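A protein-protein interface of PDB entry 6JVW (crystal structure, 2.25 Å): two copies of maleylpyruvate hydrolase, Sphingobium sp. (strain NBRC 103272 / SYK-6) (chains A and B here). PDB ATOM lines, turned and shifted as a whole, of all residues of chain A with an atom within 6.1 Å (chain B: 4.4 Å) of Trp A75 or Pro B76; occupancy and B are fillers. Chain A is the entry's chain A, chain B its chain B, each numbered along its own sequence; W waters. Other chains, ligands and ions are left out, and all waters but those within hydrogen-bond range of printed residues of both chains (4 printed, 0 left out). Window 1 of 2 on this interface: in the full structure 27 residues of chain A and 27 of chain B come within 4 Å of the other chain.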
ATOM      1  N   TRP A  33      -3.514 -20.477  17.897  1.00  0.00           N
ATOM      2  CA  TRP A  33      -3.367 -19.525  16.773  1.00  0.00           C
ATOM      3  C   TRP A  33      -4.084 -20.076  15.537  1.00  0.00           C
ATOM      4  O   TRP A  33      -3.882 -21.228  15.167  1.00  0.00           O
ATOM      5  CB  TRP A  33      -1.884 -19.251  16.504  1.00  0.00           C
ATOM      6  CG  TRP A  33      -1.774 -18.098  15.562  1.00  0.00           C
ATOM      7  CD1 TRP A  33      -1.731 -16.777  15.889  1.00  0.00           C
ATOM      8  CD2 TRP A  33      -1.902 -18.165  14.135  1.00  0.00           C
ATOM      9  NE1 TRP A  33      -1.758 -16.020  14.754  1.00  0.00           N
ATOM     10  CE2 TRP A  33      -1.852 -16.842  13.662  1.00  0.00           C
ATOM     11  CE3 TRP A  33      -2.024 -19.214  13.216  1.00  0.00           C
ATOM     12  CZ2 TRP A  33      -1.904 -16.532  12.303  1.00  0.00           C
ATOM     13  CZ3 TRP A  33      -2.085 -18.907  11.872  1.00  0.00           C
ATOM     14  CH2 TRP A  33      -2.033 -17.587  11.428  1.00  0.00           C
ATOM     15  N   PRO A  34      -4.957 -19.300  14.854  1.00  0.00           N
ATOM     16  CA  PRO A  34      -5.460 -18.023  15.362  1.00  0.00           C
ATOM     17  C   PRO A  34      -6.283 -18.146  16.661  1.00  0.00           C
ATOM     18  O   PRO A  34      -6.936 -19.170  16.867  1.00  0.00           O
ATOM     19  CB  PRO A  34      -6.355 -17.504  14.233  1.00  0.00           C
ATOM     20  CG  PRO A  34      -5.897 -18.266  13.009  1.00  0.00           C
ATOM     21  CD  PRO A  34      -5.509 -19.630  13.535  1.00  0.00           C
ATOM     22  N   ASP A  35      -6.208 -17.127  17.529  1.00  0.00           N
ATOM     23  CA  ASP A  35      -6.886 -17.153  18.853  1.00  0.00           C
ATOM     24  C   ASP A  35      -8.401 -16.943  18.674  1.00  0.00           C
ATOM     25  O   ASP A  35      -8.850 -15.810  18.370  1.00  0.00           O
ATOM     26  CB  ASP A  35      -6.214 -16.159  19.798  1.00  0.00           C
ATOM     27  CG  ASP A  35      -6.757 -16.257  21.213  1.00  0.00           C
ATOM     28  OD1 ASP A  35      -7.910 -16.790  21.382  1.00  0.00           O
ATOM     29  OD2 ASP A  35      -6.051 -15.776  22.130  1.00  0.00           O
ATOM     30  N   MET A  36      -9.193 -17.999  18.842  1.00  0.00           N
ATOM     31  CA  MET A  36     -10.666 -17.932  18.688  1.00  0.00           C
ATOM     32  C   MET A  36     -11.397 -18.291  19.993  1.00  0.00           C
ATOM     33  O   MET A  36     -12.573 -18.630  19.933  1.00  0.00           O
ATOM     34  CB  MET A  36     -11.119 -18.847  17.555  1.00  0.00           C
ATOM     35  CG  MET A  36     -10.274 -18.734  16.308  1.00  0.00           C
ATOM     36  SD  MET A  36     -10.286 -17.118  15.496  1.00  0.00           S
ATOM     37  CE  MET A  36     -11.873 -17.149  14.684  1.00  0.00           C
ATOM     38  N   ILE A  39     -14.510 -16.233  21.031  1.00  0.00           N
ATOM     39  CA  ILE A  39     -15.650 -16.485  20.109  1.00  0.00           C
ATOM     40  C   ILE A  39     -16.346 -17.776  20.550  1.00  0.00           C
ATOM     41  O   ILE A  39     -17.562 -17.773  20.662  1.00  0.00           O
ATOM     42  CB  ILE A  39     -15.156 -16.445  18.657  1.00  0.00           C
ATOM     43  CG1 ILE A  39     -14.861 -14.981  18.301  1.00  0.00           C
ATOM     44  CG2 ILE A  39     -16.156 -17.091  17.694  1.00  0.00           C
ATOM     45  CD1 ILE A  39     -14.281 -14.778  16.952  1.00  0.00           C
ATOM     46  N   VAL A  73     -11.855  -9.613  21.331  1.00  0.00           N
ATOM     47  CA  VAL A  73     -12.063 -10.494  20.144  1.00  0.00           C
ATOM     48  C   VAL A  73     -11.096 -10.146  19.029  1.00  0.00           C
ATOM     49  O   VAL A  73     -11.345  -9.225  18.263  1.00  0.00           O
ATOM     50  CB  VAL A  73     -13.494 -10.379  19.619  1.00  0.00           C
ATOM     51  CG1 VAL A  73     -13.737 -11.409  18.534  1.00  0.00           C
ATOM     52  CG2 VAL A  73     -14.513 -10.501  20.728  1.00  0.00           C
ATOM     53  N   PRO A  74      -9.980 -10.873  18.892  1.00  0.00           N
ATOM     54  CA  PRO A  74      -8.932 -10.494  17.944  1.00  0.00           C
ATOM     55  C   PRO A  74      -9.063 -10.906  16.469  1.00  0.00           C
ATOM     56  O   PRO A  74      -8.285 -10.362  15.657  1.00  0.00           O
ATOM     57  CB  PRO A  74      -7.679 -11.180  18.516  1.00  0.00           C
ATOM     58  CG  PRO A  74      -8.238 -12.396  19.209  1.00  0.00           C
ATOM     59  CD  PRO A  74      -9.570 -11.964  19.782  1.00  0.00           C
ATOM     60  N   TRP A  75      -9.991 -11.799  16.130  1.00  0.00           N
ATOM     61  CA  TRP A  75     -10.166 -12.314  14.741  1.00  0.00           C
ATOM     62  C   TRP A  75     -11.644 -12.576  14.498  1.00  0.00           C
ATOM     63  O   TRP A  75     -12.116 -13.692  14.316  1.00  0.00           O
ATOM     64  CB  TRP A  75      -9.279 -13.529  14.586  1.00  0.00           C
ATOM     65  CG  TRP A  75      -9.007 -14.028  13.210  1.00  0.00           C
ATOM     66  CD1 TRP A  75      -9.923 -14.421  12.272  1.00  0.00           C
ATOM     67  CD2 TRP A  75      -7.709 -14.314  12.662  1.00  0.00           C
ATOM     68  NE1 TRP A  75      -9.275 -14.919  11.171  1.00  0.00           N
ATOM     69  CE2 TRP A  75      -7.919 -14.868  11.382  1.00  0.00           C
ATOM     70  CE3 TRP A  75      -6.405 -14.159  13.128  1.00  0.00           C
ATOM     71  CZ2 TRP A  75      -6.870 -15.279  10.559  1.00  0.00           C
ATOM     72  CZ3 TRP A  75      -5.368 -14.559  12.318  1.00  0.00           C
ATOM     73  CH2 TRP A  75      -5.594 -15.076  11.039  1.00  0.00           C
ATOM     74  N   PRO A  76     -12.441 -11.493  14.464  1.00  0.00           N
ATOM     75  CA  PRO A  76     -13.874 -11.632  14.289  1.00  0.00           C
ATOM     76  C   PRO A  76     -14.081 -12.055  12.835  1.00  0.00           C
ATOM     77  O   PRO A  76     -13.188 -11.822  12.032  1.00  0.00           O
ATOM     78  CB  PRO A  76     -14.338 -10.226  14.662  1.00  0.00           C
ATOM     79  CG  PRO A  76     -13.237  -9.340  14.145  1.00  0.00           C
ATOM     80  CD  PRO A  76     -11.996 -10.093  14.498  1.00  0.00           C
ATOM     81  N   ASN A  77     -15.203 -12.715  12.538  1.00  0.00           N
ATOM     82  CA  ASN A  77     -15.614 -12.986  11.136  1.00  0.00           C
ATOM     83  C   ASN A  77     -15.669 -11.641  10.378  1.00  0.00           C
ATOM     84  O   ASN A  77     -15.226 -11.618   9.223  1.00  0.00           O
ATOM     85  CB  ASN A  77     -16.912 -13.798  11.085  1.00  0.00           C
ATOM     86  CG  ASN A  77     -17.293 -14.167   9.674  1.00  0.00           C
ATOM     87  OD1 ASN A  77     -18.157 -13.511   9.086  1.00  0.00           O
ATOM     88  ND2 ASN A  77     -16.619 -15.165   9.111  1.00  0.00           N
ATOM     89  N   LYS A  78     -16.181 -10.559  10.999  1.00  0.00           N
ATOM     90  CA  LYS A  78     -16.289  -9.196  10.371  1.00  0.00           C
ATOM     91  C   LYS A  78     -16.464  -8.084  11.412  1.00  0.00           C
ATOM     92  O   LYS A  78     -16.920  -8.372  12.521  1.00  0.00           O
ATOM     93  CB  LYS A  78     -17.447  -9.111   9.370  1.00  0.00           C
ATOM     94  CG  LYS A  78     -18.790  -9.652   9.840  1.00  0.00           C
ATOM     95  CD  LYS A  78     -19.604 -10.175   8.676  1.00  0.00           C
ATOM     96  CE  LYS A  78     -20.752 -11.068   9.058  1.00  0.00           C
ATOM     97  NZ  LYS A  78     -20.325 -12.239   9.862  1.00  0.00           N
ATOM     98  N   GLY A 109     -10.251  -6.991  10.446  1.00  0.00           N
ATOM     99  CA  GLY A 109      -9.798  -7.544  11.739  1.00  0.00           C
ATOM    100  C   GLY A 109      -8.394  -7.083  12.114  1.00  0.00           C
ATOM    101  O   GLY A 109      -8.129  -6.915  13.304  1.00  0.00           O
ATOM    102  N   LEU A 112      -7.774  -4.137  14.582  1.00  0.00           N
ATOM    103  CA  LEU A 112      -8.138  -4.244  16.014  1.00  0.00           C
ATOM    104  C   LEU A 112      -6.900  -4.005  16.886  1.00  0.00           C
ATOM    105  O   LEU A 112      -5.871  -4.527  16.545  1.00  0.00           O
ATOM    106  CB  LEU A 112      -8.731  -5.626  16.284  1.00  0.00           C
ATOM    107  CG  LEU A 112     -10.175  -5.806  15.831  1.00  0.00           C
ATOM    108  CD1 LEU A 112     -10.576  -7.262  15.929  1.00  0.00           C
ATOM    109  CD2 LEU A 112     -11.105  -4.936  16.629  1.00  0.00           C
ATOM    110  N   MET B  36     -10.277 -23.153  11.404  1.00  0.00           N
ATOM    111  CA  MET B  36      -9.012 -22.466  11.022  1.00  0.00           C
ATOM    112  C   MET B  36      -7.918 -23.466  10.614  1.00  0.00           C
ATOM    113  O   MET B  36      -6.739 -23.088  10.678  1.00  0.00           O
ATOM    114  CB  MET B  36      -8.481 -21.620  12.183  1.00  0.00           C
ATOM    115  CG  MET B  36      -9.528 -20.781  12.874  1.00  0.00           C
ATOM    116  SD  MET B  36     -10.426 -19.549  11.836  1.00  0.00           S
ATOM    117  CE  MET B  36      -9.109 -18.439  11.367  1.00  0.00           C
ATOM    118  N   ILE B  39      -5.773 -22.406   7.525  1.00  0.00           N
ATOM    119  CA  ILE B  39      -4.888 -21.288   7.942  1.00  0.00           C
ATOM    120  C   ILE B  39      -3.661 -21.866   8.644  1.00  0.00           C
ATOM    121  O   ILE B  39      -2.550 -21.486   8.261  1.00  0.00           O
ATOM    122  CB  ILE B  39      -5.673 -20.225   8.722  1.00  0.00           C
ATOM    123  CG1 ILE B  39      -6.504 -19.437   7.702  1.00  0.00           C
ATOM    124  CG2 ILE B  39      -4.751 -19.298   9.525  1.00  0.00           C
ATOM    125  CD1 ILE B  39      -7.460 -18.472   8.304  1.00  0.00           C
ATOM    126  N   VAL B  73     -10.608 -21.674   2.542  1.00  0.00           N
ATOM    127  CA  VAL B  73     -10.359 -20.841   3.761  1.00  0.00           C
ATOM    128  C   VAL B  73     -11.669 -20.185   4.179  1.00  0.00           C
ATOM    129  O   VAL B  73     -12.013 -19.136   3.646  1.00  0.00           O
ATOM    130  CB  VAL B  73      -9.279 -19.772   3.526  1.00  0.00           C
ATOM    131  CG1 VAL B  73      -8.942 -19.059   4.822  1.00  0.00           C
ATOM    132  CG2 VAL B  73      -8.022 -20.356   2.914  1.00  0.00           C
ATOM    133  N   PRO B  74     -12.449 -20.794   5.100  1.00  0.00           N
ATOM    134  CA  PRO B  74     -13.786 -20.296   5.410  1.00  0.00           C
ATOM    135  C   PRO B  74     -13.860 -19.063   6.320  1.00  0.00           C
ATOM    136  O   PRO B  74     -14.935 -18.467   6.376  1.00  0.00           O
ATOM    137  CB  PRO B  74     -14.451 -21.501   6.112  1.00  0.00           C
ATOM    138  CG  PRO B  74     -13.296 -22.212   6.771  1.00  0.00           C
ATOM    139  CD  PRO B  74     -12.131 -22.038   5.822  1.00  0.00           C
ATOM    140  N   TRP B  75     -12.776 -18.672   6.989  1.00  0.00           N
ATOM    141  CA  TRP B  75     -12.822 -17.528   7.948  1.00  0.00           C
ATOM    142  C   TRP B  75     -11.466 -16.835   7.932  1.00  0.00           C
ATOM    143  O   TRP B  75     -10.667 -16.945   8.856  1.00  0.00           O
ATOM    144  CB  TRP B  75     -13.242 -18.085   9.299  1.00  0.00           C
ATOM    145  CG  TRP B  75     -13.570 -17.166  10.419  1.00  0.00           C
ATOM    146  CD1 TRP B  75     -12.796 -16.180  10.961  1.00  0.00           C
ATOM    147  CD2 TRP B  75     -14.718 -17.302  11.278  1.00  0.00           C
ATOM    148  NE1 TRP B  75     -13.412 -15.667  12.081  1.00  0.00           N
ATOM    149  CE2 TRP B  75     -14.593 -16.328  12.296  1.00  0.00           C
ATOM    150  CE3 TRP B  75     -15.853 -18.125  11.265  1.00  0.00           C
ATOM    151  CZ2 TRP B  75     -15.549 -16.157  13.294  1.00  0.00           C
ATOM    152  CZ3 TRP B  75     -16.796 -17.962  12.263  1.00  0.00           C
ATOM    153  CH2 TRP B  75     -16.652 -16.982  13.253  1.00  0.00           C
ATOM    154  N   PRO B  76     -11.142 -16.165   6.803  1.00  0.00           N
ATOM    155  CA  PRO B  76      -9.857 -15.500   6.656  1.00  0.00           C
ATOM    156  C   PRO B  76      -9.884 -14.275   7.575  1.00  0.00           C
ATOM    157  O   PRO B  76     -10.989 -13.840   7.969  1.00  0.00           O
ATOM    158  CB  PRO B  76      -9.824 -15.160   5.162  1.00  0.00           C
ATOM    159  CG  PRO B  76     -11.278 -14.917   4.827  1.00  0.00           C
ATOM    160  CD  PRO B  76     -12.034 -15.931   5.661  1.00  0.00           C
ATOM    161  N   ASN B  77      -8.716 -13.713   7.890  1.00  0.00           N
ATOM    162  CA  ASN B  77      -8.659 -12.460   8.687  1.00  0.00           C
ATOM    163  C   ASN B  77      -9.297 -11.343   7.836  1.00  0.00           C
ATOM    164  O   ASN B  77      -9.949 -10.464   8.425  1.00  0.00           O
ATOM    165  CB  ASN B  77      -7.232 -12.178   9.154  1.00  0.00           C
ATOM    166  CG  ASN B  77      -7.104 -10.891   9.943  1.00  0.00           C
ATOM    167  OD1 ASN B  77      -6.765  -9.860   9.367  1.00  0.00           O
ATOM    168  ND2 ASN B  77      -7.449 -10.926  11.223  1.00  0.00           N
ATOM    169  N   LYS B  78      -9.148 -11.388   6.502  1.00  0.00           N
ATOM    170  CA  LYS B  78      -9.730 -10.386   5.581  1.00  0.00           C
ATOM    171  C   LYS B  78      -9.739 -10.888   4.137  1.00  0.00           C
ATOM    172  O   LYS B  78      -8.995 -11.829   3.812  1.00  0.00           O
ATOM    173  CB  LYS B  78      -8.988  -9.053   5.658  1.00  0.00           C
ATOM    174  CG  LYS B  78      -7.467  -9.098   5.551  1.00  0.00           C
ATOM    175  CD  LYS B  78      -6.876  -7.809   6.140  1.00  0.00           C
ATOM    176  CE  LYS B  78      -5.449  -7.916   6.627  1.00  0.00           C
ATOM    177  NZ  LYS B  78      -5.197  -9.137   7.439  1.00  0.00           N
ATOM    178  N   ILE B  79     -10.585 -10.245   3.335  1.00  0.00           N
ATOM    179  CA  ILE B  79     -10.676 -10.400   1.865  1.00  0.00           C
ATOM    180  C   ILE B  79     -10.553  -9.015   1.261  1.00  0.00           C
ATOM    181  O   ILE B  79     -11.458  -8.187   1.497  1.00  0.00           O
ATOM    182  CB  ILE B  79     -11.992 -11.063   1.417  1.00  0.00           C
ATOM    183  CG1 ILE B  79     -12.236 -12.385   2.143  1.00  0.00           C
ATOM    184  CG2 ILE B  79     -11.967 -11.222  -0.093  1.00  0.00           C
ATOM    185  CD1 ILE B  79     -13.648 -12.925   1.987  1.00  0.00           C
ATOM    186  N   LEU B 112     -18.187 -15.772   1.657  1.00  0.00           N
ATOM    187  CA  LEU B 112     -17.421 -16.879   1.035  1.00  0.00           C
ATOM    188  C   LEU B 112     -18.396 -18.013   0.761  1.00  0.00           C
ATOM    189  O   LEU B 112     -19.308 -18.206   1.550  1.00  0.00           O
ATOM    190  CB  LEU B 112     -16.267 -17.364   1.924  1.00  0.00           C
ATOM    191  CG  LEU B 112     -15.054 -16.440   1.979  1.00  0.00           C
ATOM    192  CD1 LEU B 112     -14.117 -16.835   3.110  1.00  0.00           C
ATOM    193  CD2 LEU B 112     -14.319 -16.394   0.665  1.00  0.00           C
ATOM    194  N   GLN B 237      -2.203 -11.765   6.903  1.00  0.00           N
ATOM    195  CA  GLN B 237      -2.191 -13.044   7.654  1.00  0.00           C
ATOM    196  C   GLN B 237      -2.241 -14.181   6.639  1.00  0.00           C
ATOM    197  O   GLN B 237      -2.828 -14.052   5.554  1.00  0.00           O
ATOM    198  CB  GLN B 237      -3.341 -13.127   8.680  1.00  0.00           C
ATOM    199  CG  GLN B 237      -3.282 -12.091   9.794  1.00  0.00           C
ATOM    200  CD  GLN B 237      -2.106 -12.210  10.739  1.00  0.00           C
ATOM    201  OE1 GLN B 237      -1.361 -13.179  10.722  1.00  0.00           O
ATOM    202  NE2 GLN B 237      -1.911 -11.199  11.574  1.00  0.00           N
ATOM    203  N   GLY B 239      -3.765 -17.236   4.940  1.00  0.00           N
ATOM    204  CA  GLY B 239      -5.169 -17.457   4.556  1.00  0.00           C
ATOM    205  C   GLY B 239      -5.839 -16.209   3.994  1.00  0.00           C
ATOM    206  O   GLY B 239      -6.912 -16.369   3.410  1.00  0.00           O
ATOM    207  N   ILE B 241      -7.153 -13.417   1.579  1.00  0.00           N
ATOM    208  CA  ILE B 241      -7.495 -13.528   0.139  1.00  0.00           C
ATOM    209  C   ILE B 241      -7.356 -12.128  -0.457  1.00  0.00           C
ATOM    210  O   ILE B 241      -7.966 -11.220   0.085  1.00  0.00           O
ATOM    211  CB  ILE B 241      -8.893 -14.154  -0.018  1.00  0.00           C
ATOM    212  CG1 ILE B 241      -8.928 -15.585   0.533  1.00  0.00           C
ATOM    213  CG2 ILE B 241      -9.351 -14.096  -1.464  1.00  0.00           C
ATOM    214  CD1 ILE B 241     -10.305 -16.107   0.860  1.00  0.00           C
HETATM  215  O   HOH W   1     -16.882 -16.988   6.745  1.00  0.00           O
HETATM  216  O   HOH W   2     -13.714 -13.886   7.803  1.00  0.00           O
HETATM  217  O   HOH W   3     -10.941 -10.495  10.922  1.00  0.00           O
HETATM  218  O   HOH W   4      -6.994  -9.421  13.664  1.00  0.00           O
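The backbone NH (N) of Asn A77 sits close to the indole nitrogen (NE1) of Trp B75.
The backbone carbonyl oxygen (O) of Trp A75 lies within hydrogen-bond range of the indole nitrogen (NE1) of Trp B75 (3.3 Å).
OD1 of Asn A77 is in hydrogen-bond range of NZ of Lys A78 (2.6 Å).
OD1 of Asn B77 lies within hydrogen-bond range of NZ of Lys B78.
Among the printed residues, merely in contact across the chains: Met A36 with Trp B75 (3.4 Å), Trp A75 with Asn B77 (3.4 Å), Trp A75 with Met B36 (3.5 Å), Trp A33 with Ile B39 (3.6 Å), Pro A34 with Met B36 (3.6 Å), Trp A75 with Pro B76 (3.7 Å), Trp A33 with Gln B237 (3.7 Å), Pro A76 with Trp B75 (3.8 Å), Trp A75 with Gln B237 (3.8 Å), Pro A34 with Ile B39 (3.8 Å), Trp A75 with Ile B39 (3.95 Å) and Met A36 with Met B36 (3.996 Å).
Pro A74 touches none of the printed residues of chain B.
Trp A75 touches just these residues of chain B: Met B36, Ile B39, Trp B75, Pro B76, Asn B77 and Gln B237.
Of the printed residues of chain B, Pro A76 touches Trp B75.
Of the printed residues of chain B, Asn A77 touches Trp B75 (3.5 Å).
Of the printed residues of chain A, Trp B75 touches Met A36, Trp A75, Pro A76 and Asn A77.
Pro B76 touches just one residue of chain A: Trp A75 (3.7 Å).
The nearest residue of chain A that does not touch Pro B76 is Asn A77 (4.9 Å).
Of the 13 printed residues of chain B, 6 touch a printed residue of chain A.
Hydrophobic or aromatic side chains of chain B within 4 Å of the printed part of chain A: Met B36, Ile B39 and Trp B75.
Of the 13 printed residues of chain A, 6 touch a printed residue of chain B.
Printed residues of chain A that touch a printed residue of chain B: Trp A33, Pro A34, Met A36, Trp A75, Pro A76 and Asn A77.
Hydrophobic or aromatic side chains of chain A that line the printed part of chain B: Trp A33, Pro A34, Met A36 and Trp A75.
Among the printed residues, 14 pairs touch across the chains.
Trp A75 touches Ile B39, but with the chains exchanged Ile A39 does not touch Trp B75 (4.1 Å).
Trp A75 touches its own counterpart, Trp B75.
Trp A75 touches Pro B76, and with the chains exchanged Pro A76 touches Trp B75.
Trp A75 touches Asn B77, and with the chains exchanged Asn A77 touches Trp B75.
Positions printed for both chains: 36, 39, 73, 74, 75, 76, 77, 78 and 112.
Water W1 lies within hydrogen-bond range of O of Pro B74 (2.5 Å) and ND2 of Asn A77 (3.0 Å).
Water W4 lies within hydrogen-bond range of O of Pro A74 (2.6 Å), O of Gly A109 (2.8 Å) and ND2 of Asn B77 (2.9 Å).
Water W3 lies within hydrogen-bond range of the backbone carbonyl oxygen (O) of Asn B77 (2.7 Å) and the backbone carbonyl oxygen (O) of Pro A76 (2.8 Å).
Water W2 bridges O of Pro B76 (2.7 Å) and O of Asn A77 (3.1 Å).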
